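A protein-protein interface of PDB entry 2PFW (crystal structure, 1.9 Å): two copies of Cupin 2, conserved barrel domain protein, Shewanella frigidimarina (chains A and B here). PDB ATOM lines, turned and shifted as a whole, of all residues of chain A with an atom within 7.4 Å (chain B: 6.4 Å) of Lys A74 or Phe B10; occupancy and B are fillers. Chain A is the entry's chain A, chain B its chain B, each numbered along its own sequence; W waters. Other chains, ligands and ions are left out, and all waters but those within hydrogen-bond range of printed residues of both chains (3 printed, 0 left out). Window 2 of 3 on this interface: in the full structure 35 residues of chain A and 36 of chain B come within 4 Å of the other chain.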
ATOM      1  N   PHE A  65      21.153  -1.563  11.738  1.00  0.00           N
ATOM      2  CA  PHE A  65      20.776  -0.151  11.745  1.00  0.00           C
ATOM      3  C   PHE A  65      21.961   0.704  11.290  1.00  0.00           C
ATOM      4  O   PHE A  65      23.025   0.654  11.903  1.00  0.00           O
ATOM      5  CB  PHE A  65      20.292   0.294  13.126  1.00  0.00           C
ATOM      6  CG  PHE A  65      18.847  -0.124  13.367  1.00  0.00           C
ATOM      7  CD1 PHE A  65      18.556  -1.393  13.842  1.00  0.00           C
ATOM      8  CD2 PHE A  65      17.809   0.751  13.112  1.00  0.00           C
ATOM      9  CE1 PHE A  65      17.243  -1.767  14.048  1.00  0.00           C
ATOM     10  CE2 PHE A  65      16.494   0.384  13.319  1.00  0.00           C
ATOM     11  CZ  PHE A  65      16.213  -0.885  13.793  1.00  0.00           C
ATOM     12  N   HIS A  66      21.746   1.453  10.216  1.00  0.00           N
ATOM     13  CA  HIS A  66      22.656   2.506   9.788  1.00  0.00           C
ATOM     14  C   HIS A  66      22.301   3.777  10.563  1.00  0.00           C
ATOM     15  O   HIS A  66      21.277   4.391  10.265  1.00  0.00           O
ATOM     16  CB  HIS A  66      22.567   2.769   8.287  1.00  0.00           C
ATOM     17  CG  HIS A  66      23.128   1.687   7.421  1.00  0.00           C
ATOM     18  ND1 HIS A  66      22.585   0.423   7.383  1.00  0.00           N
ATOM     19  CD2 HIS A  66      24.169   1.664   6.553  1.00  0.00           C
ATOM     20  CE1 HIS A  66      23.265  -0.331   6.537  1.00  0.00           C
ATOM     21  NE2 HIS A  66      24.236   0.402   6.020  1.00  0.00           N
ATOM     22  N   VAL A  67      23.113   4.153  11.541  1.00  0.00           N
ATOM     23  CA  VAL A  67      22.716   5.290  12.375  1.00  0.00           C
ATOM     24  C   VAL A  67      23.670   6.470  12.197  1.00  0.00           C
ATOM     25  O   VAL A  67      24.891   6.329  12.260  1.00  0.00           O
ATOM     26  CB  VAL A  67      22.627   4.913  13.864  1.00  0.00           C
ATOM     27  CG1 VAL A  67      22.256   6.139  14.686  1.00  0.00           C
ATOM     28  CG2 VAL A  67      21.607   3.802  14.064  1.00  0.00           C
ATOM     29  N   ASN A  68      23.086   7.648  11.968  1.00  0.00           N
ATOM     30  CA  ASN A  68      23.866   8.882  11.944  1.00  0.00           C
ATOM     31  C   ASN A  68      23.630   9.684  13.225  1.00  0.00           C
ATOM     32  O   ASN A  68      22.482  10.054  13.475  1.00  0.00           O
ATOM     33  CB  ASN A  68      23.515   9.735  10.722  1.00  0.00           C
ATOM     34  CG  ASN A  68      24.525  10.857  10.529  1.00  0.00           C
ATOM     35  OD1 ASN A  68      25.148  11.328  11.483  1.00  0.00           O
ATOM     36  ND2 ASN A  68      24.699  11.288   9.282  1.00  0.00           N
ATOM     37  N   VAL A  69      24.685   9.923  13.985  1.00  0.00           N
ATOM     38  CA  VAL A  69      24.664  10.897  15.070  1.00  0.00           C
ATOM     39  C   VAL A  69      25.744  11.962  14.861  1.00  0.00           C
ATOM     40  O   VAL A  69      26.932  11.658  14.887  1.00  0.00           O
ATOM     41  CB  VAL A  69      24.856  10.257  16.453  1.00  0.00           C
ATOM     42  CG1 VAL A  69      24.827  11.334  17.530  1.00  0.00           C
ATOM     43  CG2 VAL A  69      23.779   9.219  16.724  1.00  0.00           C
ATOM     44  N   GLY A  71      26.820  13.502  12.420  1.00  0.00           N
ATOM     45  CA  GLY A  71      27.641  13.283  11.245  1.00  0.00           C
ATOM     46  C   GLY A  71      28.500  12.040  11.350  1.00  0.00           C
ATOM     47  O   GLY A  71      29.034  11.553  10.352  1.00  0.00           O
ATOM     48  N   VAL A  72      28.651  11.490  12.552  1.00  0.00           N
ATOM     49  CA  VAL A  72      29.317  10.189  12.696  1.00  0.00           C
ATOM     50  C   VAL A  72      28.371   9.073  12.273  1.00  0.00           C
ATOM     51  O   VAL A  72      27.183   9.102  12.596  1.00  0.00           O
ATOM     52  CB  VAL A  72      29.802   9.982  14.135  1.00  0.00           C
ATOM     53  CG1 VAL A  72      30.618   8.708  14.265  1.00  0.00           C
ATOM     54  CG2 VAL A  72      30.625  11.181  14.593  1.00  0.00           C
ATOM     55  N   ILE A  73      28.864   8.088  11.522  1.00  0.00           N
ATOM     56  CA  ILE A  73      27.967   7.078  10.966  1.00  0.00           C
ATOM     57  C   ILE A  73      28.468   5.675  11.299  1.00  0.00           C
ATOM     58  O   ILE A  73      29.634   5.328  11.098  1.00  0.00           O
ATOM     59  CB  ILE A  73      27.805   7.170   9.438  1.00  0.00           C
ATOM     60  CG1 ILE A  73      27.448   8.556   8.906  1.00  0.00           C
ATOM     61  CG2 ILE A  73      26.786   6.129   8.983  1.00  0.00           C
ATOM     62  CD1 ILE A  73      26.077   8.637   8.278  1.00  0.00           C
ATOM     63  N   LYS A  74      27.579   4.835  11.834  1.00  0.00           N
ATOM     64  CA  LYS A  74      28.001   3.467  12.148  1.00  0.00           C
ATOM     65  C   LYS A  74      26.877   2.504  11.774  1.00  0.00           C
ATOM     66  O   LYS A  74      25.703   2.871  11.796  1.00  0.00           O
ATOM     67  CB  LYS A  74      28.411   3.309  13.607  1.00  0.00           C
ATOM     68  CG  LYS A  74      29.218   4.411  14.246  1.00  0.00           C
ATOM     69  CD  LYS A  74      30.612   4.044  14.686  1.00  0.00           C
ATOM     70  CE  LYS A  74      31.554   5.231  14.722  1.00  0.00           C
ATOM     71  NZ  LYS A  74      32.987   4.841  14.637  1.00  0.00           N
ATOM     72  N   VAL A  75      27.236   1.272  11.416  1.00  0.00           N
ATOM     73  CA  VAL A  75      26.234   0.221  11.265  1.00  0.00           C
ATOM     74  C   VAL A  75      26.075  -0.498  12.606  1.00  0.00           C
ATOM     75  O   VAL A  75      27.079  -0.946  13.153  1.00  0.00           O
ATOM     76  CB  VAL A  75      26.622  -0.786  10.175  1.00  0.00           C
ATOM     77  CG1 VAL A  75      25.540  -1.843  10.029  1.00  0.00           C
ATOM     78  CG2 VAL A  75      26.873  -0.056   8.864  1.00  0.00           C
ATOM     79  N   LEU A  76      24.850  -0.583  13.093  1.00  0.00           N
ATOM     80  CA  LEU A  76      24.588  -1.170  14.403  1.00  0.00           C
ATOM     81  C   LEU A  76      23.748  -2.440  14.257  1.00  0.00           C
ATOM     82  O   LEU A  76      22.839  -2.499  13.431  1.00  0.00           O
ATOM     83  CB  LEU A  76      23.863  -0.196  15.330  1.00  0.00           C
ATOM     84  CG  LEU A  76      24.549   1.127  15.671  1.00  0.00           C
ATOM     85  CD1 LEU A  76      23.886   1.767  16.884  1.00  0.00           C
ATOM     86  CD2 LEU A  76      26.035   0.943  15.909  1.00  0.00           C
ATOM     87  N   THR A  77      24.056  -3.432  15.084  1.00  0.00           N
ATOM     88  CA  THR A  77      23.271  -4.666  15.129  1.00  0.00           C
ATOM     89  C   THR A  77      22.782  -4.941  16.548  1.00  0.00           C
ATOM     90  O   THR A  77      23.034  -4.157  17.469  1.00  0.00           O
ATOM     91  CB  THR A  77      24.107  -5.837  14.572  1.00  0.00           C
ATOM     92  OG1 THR A  77      23.289  -7.002  14.435  1.00  0.00           O
ATOM     93  CG2 THR A  77      25.243  -6.185  15.512  1.00  0.00           C
ATOM     94  N   ALA A  78      22.072  -6.045  16.721  1.00  0.00           N
ATOM     95  CA  ALA A  78      21.496  -6.437  17.999  1.00  0.00           C
ATOM     96  C   ALA A  78      22.509  -6.337  19.132  1.00  0.00           C
ATOM     97  O   ALA A  78      23.644  -6.807  19.031  1.00  0.00           O
ATOM     98  CB  ALA A  78      20.931  -7.849  17.903  1.00  0.00           C
ATOM     99  N   GLY A  79      22.100  -5.690  20.224  1.00  0.00           N
ATOM    100  CA  GLY A  79      22.932  -5.523  21.403  1.00  0.00           C
ATOM    101  C   GLY A  79      23.694  -4.213  21.408  1.00  0.00           C
ATOM    102  O   GLY A  79      24.380  -3.874  22.376  1.00  0.00           O
ATOM    103  N   ASP A  80      23.611  -3.438  20.328  1.00  0.00           N
ATOM    104  CA  ASP A  80      24.369  -2.192  20.255  1.00  0.00           C
ATOM    105  C   ASP A  80      23.465  -1.038  20.684  1.00  0.00           C
ATOM    106  O   ASP A  80      22.241  -1.178  20.719  1.00  0.00           O
ATOM    107  CB  ASP A  80      24.903  -1.918  18.860  1.00  0.00           C
ATOM    108  CG  ASP A  80      26.003  -2.809  18.353  1.00  0.00           C
ATOM    109  OD1 ASP A  80      26.819  -3.348  19.125  1.00  0.00           O
ATOM    110  OD2 ASP A  80      26.076  -2.965  17.109  1.00  0.00           O
ATOM    111  N   SER A  81      24.052   0.116  20.997  1.00  0.00           N
ATOM    112  CA  SER A  81      23.196   1.257  21.331  1.00  0.00           C
ATOM    113  C   SER A  81      23.788   2.580  20.850  1.00  0.00           C
ATOM    114  O   SER A  81      24.976   2.684  20.547  1.00  0.00           O
ATOM    115  CB  SER A  81      22.969   1.298  22.850  1.00  0.00           C
ATOM    116  OG  SER A  81      24.217   1.299  23.514  1.00  0.00           O
ATOM    117  N   PHE A  82      22.952   3.619  20.792  1.00  0.00           N
ATOM    118  CA  PHE A  82      23.480   4.968  20.582  1.00  0.00           C
ATOM    119  C   PHE A  82      22.798   5.969  21.523  1.00  0.00           C
ATOM    120  O   PHE A  82      21.716   5.706  22.036  1.00  0.00           O
ATOM    121  CB  PHE A  82      23.314   5.437  19.147  1.00  0.00           C
ATOM    122  CG  PHE A  82      21.931   5.363  18.551  1.00  0.00           C
ATOM    123  CD1 PHE A  82      21.459   4.170  18.017  1.00  0.00           C
ATOM    124  CD2 PHE A  82      21.104   6.470  18.510  1.00  0.00           C
ATOM    125  CE1 PHE A  82      20.198   4.103  17.463  1.00  0.00           C
ATOM    126  CE2 PHE A  82      19.841   6.405  17.962  1.00  0.00           C
ATOM    127  CZ  PHE A  82      19.378   5.216  17.432  1.00  0.00           C
ATOM    128  N   GLY A  91      20.136  10.452  12.440  1.00  0.00           N
ATOM    129  CA  GLY A  91      19.240   9.677  11.588  1.00  0.00           C
ATOM    130  C   GLY A  91      19.415   8.175  11.779  1.00  0.00           C
ATOM    131  O   GLY A  91      20.473   7.761  12.246  1.00  0.00           O
ATOM    132  N   VAL A  93      18.351   4.373   9.648  1.00  0.00           N
ATOM    133  CA  VAL A  93      17.807   3.574   8.564  1.00  0.00           C
ATOM    134  C   VAL A  93      17.977   2.081   8.829  1.00  0.00           C
ATOM    135  O   VAL A  93      19.033   1.667   9.291  1.00  0.00           O
ATOM    136  CB  VAL A  93      18.511   3.901   7.225  1.00  0.00           C
ATOM    137  CG1 VAL A  93      18.540   2.689   6.312  1.00  0.00           C
ATOM    138  CG2 VAL A  93      17.816   5.073   6.555  1.00  0.00           C
ATOM    139  N   PHE B   8      27.836   6.415  20.347  1.00  0.00           N
ATOM    140  CA  PHE B   8      27.681   5.044  19.883  1.00  0.00           C
ATOM    141  C   PHE B   8      28.277   4.068  20.889  1.00  0.00           C
ATOM    142  O   PHE B   8      29.343   4.300  21.457  1.00  0.00           O
ATOM    143  CB  PHE B   8      28.334   4.851  18.510  1.00  0.00           C
ATOM    144  CG  PHE B   8      27.607   5.577  17.385  1.00  0.00           C
ATOM    145  CD1 PHE B   8      26.450   5.066  16.835  1.00  0.00           C
ATOM    146  CD2 PHE B   8      28.097   6.776  16.890  1.00  0.00           C
ATOM    147  CE1 PHE B   8      25.787   5.726  15.815  1.00  0.00           C
ATOM    148  CE2 PHE B   8      27.442   7.440  15.873  1.00  0.00           C
ATOM    149  CZ  PHE B   8      26.283   6.924  15.332  1.00  0.00           C
ATOM    150  N   SER B   9      27.590   2.947  21.120  1.00  0.00           N
ATOM    151  CA  SER B   9      28.137   1.941  22.035  1.00  0.00           C
ATOM    152  C   SER B   9      27.916   0.534  21.488  1.00  0.00           C
ATOM    153  O   SER B   9      26.894   0.292  20.856  1.00  0.00           O
ATOM    154  CB  SER B   9      27.514   2.100  23.421  1.00  0.00           C
ATOM    155  OG  SER B   9      28.219   3.108  24.139  1.00  0.00           O
ATOM    156  N   PHE B  10      28.870  -0.349  21.733  1.00  0.00           N
ATOM    157  CA  PHE B  10      28.960  -1.641  21.058  1.00  0.00           C
ATOM    158  C   PHE B  10      28.919  -2.782  22.064  1.00  0.00           C
ATOM    159  O   PHE B  10      29.783  -2.831  22.935  1.00  0.00           O
ATOM    160  CB  PHE B  10      30.243  -1.692  20.210  1.00  0.00           C
ATOM    161  CG  PHE B  10      30.151  -0.654  19.088  1.00  0.00           C
ATOM    162  CD1 PHE B  10      29.113  -0.730  18.178  1.00  0.00           C
ATOM    163  CD2 PHE B  10      31.078   0.365  18.983  1.00  0.00           C
ATOM    164  CE1 PHE B  10      28.991   0.199  17.166  1.00  0.00           C
ATOM    165  CE2 PHE B  10      30.966   1.299  17.966  1.00  0.00           C
ATOM    166  CZ  PHE B  10      29.921   1.214  17.066  1.00  0.00           C
ATOM    167  N   GLY B  11      27.934  -3.656  21.925  1.00  0.00           N
ATOM    168  CA  GLY B  11      27.683  -4.761  22.826  1.00  0.00           C
ATOM    169  C   GLY B  11      28.889  -5.642  23.057  1.00  0.00           C
ATOM    170  O   GLY B  11      29.071  -6.163  24.158  1.00  0.00           O
ATOM    171  N   GLU B  12      29.727  -5.821  22.039  1.00  0.00           N
ATOM    172  CA  GLU B  12      30.920  -6.646  22.152  1.00  0.00           C
ATOM    173  C   GLU B  12      32.116  -5.877  22.692  1.00  0.00           C
ATOM    174  O   GLU B  12      33.166  -6.457  22.985  1.00  0.00           O
ATOM    175  CB  GLU B  12      31.280  -7.244  20.783  1.00  0.00           C
ATOM    176  CG  GLU B  12      30.185  -8.109  20.182  1.00  0.00           C
ATOM    177  CD  GLU B  12      29.884  -9.341  21.016  1.00  0.00           C
ATOM    178  OE1 GLU B  12      30.834 -10.086  21.345  1.00  0.00           O
ATOM    179  OE2 GLU B  12      28.696  -9.558  21.339  1.00  0.00           O
ATOM    180  N   GLN B  13      32.004  -4.559  22.836  1.00  0.00           N
ATOM    181  CA  GLN B  13      33.149  -3.792  23.328  1.00  0.00           C
ATOM    182  C   GLN B  13      32.916  -3.193  24.709  1.00  0.00           C
ATOM    183  O   GLN B  13      33.832  -3.158  25.532  1.00  0.00           O
ATOM    184  CB  GLN B  13      33.499  -2.676  22.333  1.00  0.00           C
ATOM    185  CG  GLN B  13      33.590  -3.180  20.897  1.00  0.00           C
ATOM    186  CD  GLN B  13      34.644  -2.439  20.095  1.00  0.00           C
ATOM    187  OE1 GLN B  13      34.325  -1.510  19.354  1.00  0.00           O
ATOM    188  NE2 GLN B  13      35.893  -2.865  20.263  1.00  0.00           N
ATOM    189  N   THR B  14      31.706  -2.710  24.983  1.00  0.00           N
ATOM    190  CA  THR B  14      31.445  -2.116  26.291  1.00  0.00           C
ATOM    191  C   THR B  14      31.748  -3.124  27.400  1.00  0.00           C
ATOM    192  O   THR B  14      31.272  -4.256  27.358  1.00  0.00           O
ATOM    193  CB  THR B  14      29.996  -1.635  26.423  1.00  0.00           C
ATOM    194  OG1 THR B  14      29.709  -0.700  25.373  1.00  0.00           O
ATOM    195  CG2 THR B  14      29.790  -0.897  27.738  1.00  0.00           C
ATOM    196  N   GLU B  15      32.540  -2.701  28.381  1.00  0.00           N
ATOM    197  CA  GLU B  15      32.905  -3.593  29.479  1.00  0.00           C
ATOM    198  C   GLU B  15      31.671  -3.952  30.304  1.00  0.00           C
ATOM    199  O   GLU B  15      30.859  -3.097  30.667  1.00  0.00           O
ATOM    200  CB  GLU B  15      33.984  -2.968  30.357  1.00  0.00           C
ATOM    201  CG  GLU B  15      34.427  -3.865  31.504  1.00  0.00           C
ATOM    202  CD  GLU B  15      33.800  -3.456  32.823  1.00  0.00           C
ATOM    203  OE1 GLU B  15      32.587  -3.152  32.856  1.00  0.00           O
ATOM    204  OE2 GLU B  15      34.538  -3.443  33.836  1.00  0.00           O
ATOM    205  N   GLN B  26      26.099  -3.508  31.985  1.00  0.00           N
ATOM    206  CA  GLN B  26      26.766  -2.892  30.844  1.00  0.00           C
ATOM    207  C   GLN B  26      26.114  -1.565  30.474  1.00  0.00           C
ATOM    208  O   GLN B  26      24.900  -1.501  30.263  1.00  0.00           O
ATOM    209  CB  GLN B  26      26.731  -3.835  29.641  1.00  0.00           C
ATOM    210  CG  GLN B  26      27.519  -3.360  28.432  1.00  0.00           C
ATOM    211  CD  GLN B  26      27.303  -4.261  27.229  1.00  0.00           C
ATOM    212  OE1 GLN B  26      26.172  -4.541  26.841  1.00  0.00           O
ATOM    213  NE2 GLN B  26      28.399  -4.719  26.641  1.00  0.00           N
HETATM  214  O   HOH W   1      24.738  -5.562  24.451  1.00  0.00           O
HETATM  215  O   HOH W   2      28.713  -5.084  19.378  1.00  0.00           O
HETATM  216  O   HOH W   3      25.624  -1.338  23.555  1.00  0.00           O
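Water W2 lies within hydrogen-bond range of OD1 of Asp A80 (2.6 Å), N of Glu B12 (2.9 Å) and N of Gly B11 (3.0 Å).
Water W1 lies within hydrogen-bond range of the backbone carbonyl oxygen (O) of Gly A79 (2.7 Å) and the side-chain amide oxygen (OE1) of Gln B26 (3.0 Å).
Water W3 lies within hydrogen-bond range of the side-chain hydroxyl of Ser A81 (3.0 Å), the backbone carbonyl oxygen of Gly A79 (3.1 Å) and the backbone carbonyl oxygen of Ser B9 (3.4 Å).
O of Ser A81 lies within hydrogen-bond range of N of Ser B9, 2.7 Å away.
The side-chain carboxylate of Asp A80 lies within hydrogen-bond range of the backbone NH of Gly B11, 3.0 Å away.
Of the 19 printed residues of chain A, 9 touch a printed residue of chain B.
Hydrophobic or aromatic side chains of chain A that line the printed part of chain B: Val A67, Val A69, Val A72, Leu A76 and Phe A82.
Along chain A the printed residues that touch a printed residue of chain B span positions 67 to 82.
Among the printed residues, no Asp or Glu carboxylate lies within 4 Å of a Lys or Arg side-chain nitrogen of the other chain.
Among the printed residues, merely in contact across the chains: Val A67 with Phe B8, Val A69 with Phe B8, Val A72 with Phe B8, Lys A74 with Phe B8, Lys A74 with Phe B10, Leu A76 with Phe B10, Gly A79 with Gly B11, Asp A80 with Ser B9, Asp A80 with Phe B10, Ser A81 with Phe B8 and Phe A82 with Phe B8.
Printed residues of chain B within 4 Å of Val A67: Phe B8 (3.4 Å).
Printed residues of chain B within 4 Å of Val A69: Phe B8 (3.7 Å).
Of chain B, only Phe B8 and Phe B10 come within 4 Å of Lys A74.
Printed residues of chain B within 4 Å of Leu A76: Phe B10 (3.3 Å).
Of the printed residues of chain A, Phe B8 touches Val A67, Val A69, Val A72, Lys A74, Ser A81 and Phe A82.
Phe B10 touches just these residues of chain A: Lys A74 (3.8 Å), Leu A76 (3.3 Å) and Asp A80 (3.4 Å).
O of Gly B11 lies within hydrogen-bond range of NE2 of Gln B26.
N of Leu A76 lies within hydrogen-bond range of O of Phe A65 (2.5 Å).
The backbone carbonyl oxygen (O) of Lys A74 lies within hydrogen-bond range of the backbone NH (N) of Val A67, at 2.9 Å.
The side-chain carboxylate (OD2) of Asp A80 sits at hydrogen-bond distance from the backbone NH (N) of Thr A77 (2.9 Å).
The backbone carbonyl oxygen (O) of Phe B10 lies within hydrogen-bond range of the side-chain hydroxyl (OG1) of Thr B14 (3.2 Å).
The side-chain amide oxygen (OD1) of Asn A68 sits close to the backbone carbonyl oxygen (O) of Val A72.
No position is printed for both chains.
Of the 13 pairs that touch across the chains among the printed residues, none has its exchanged pair printed and touching as well.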
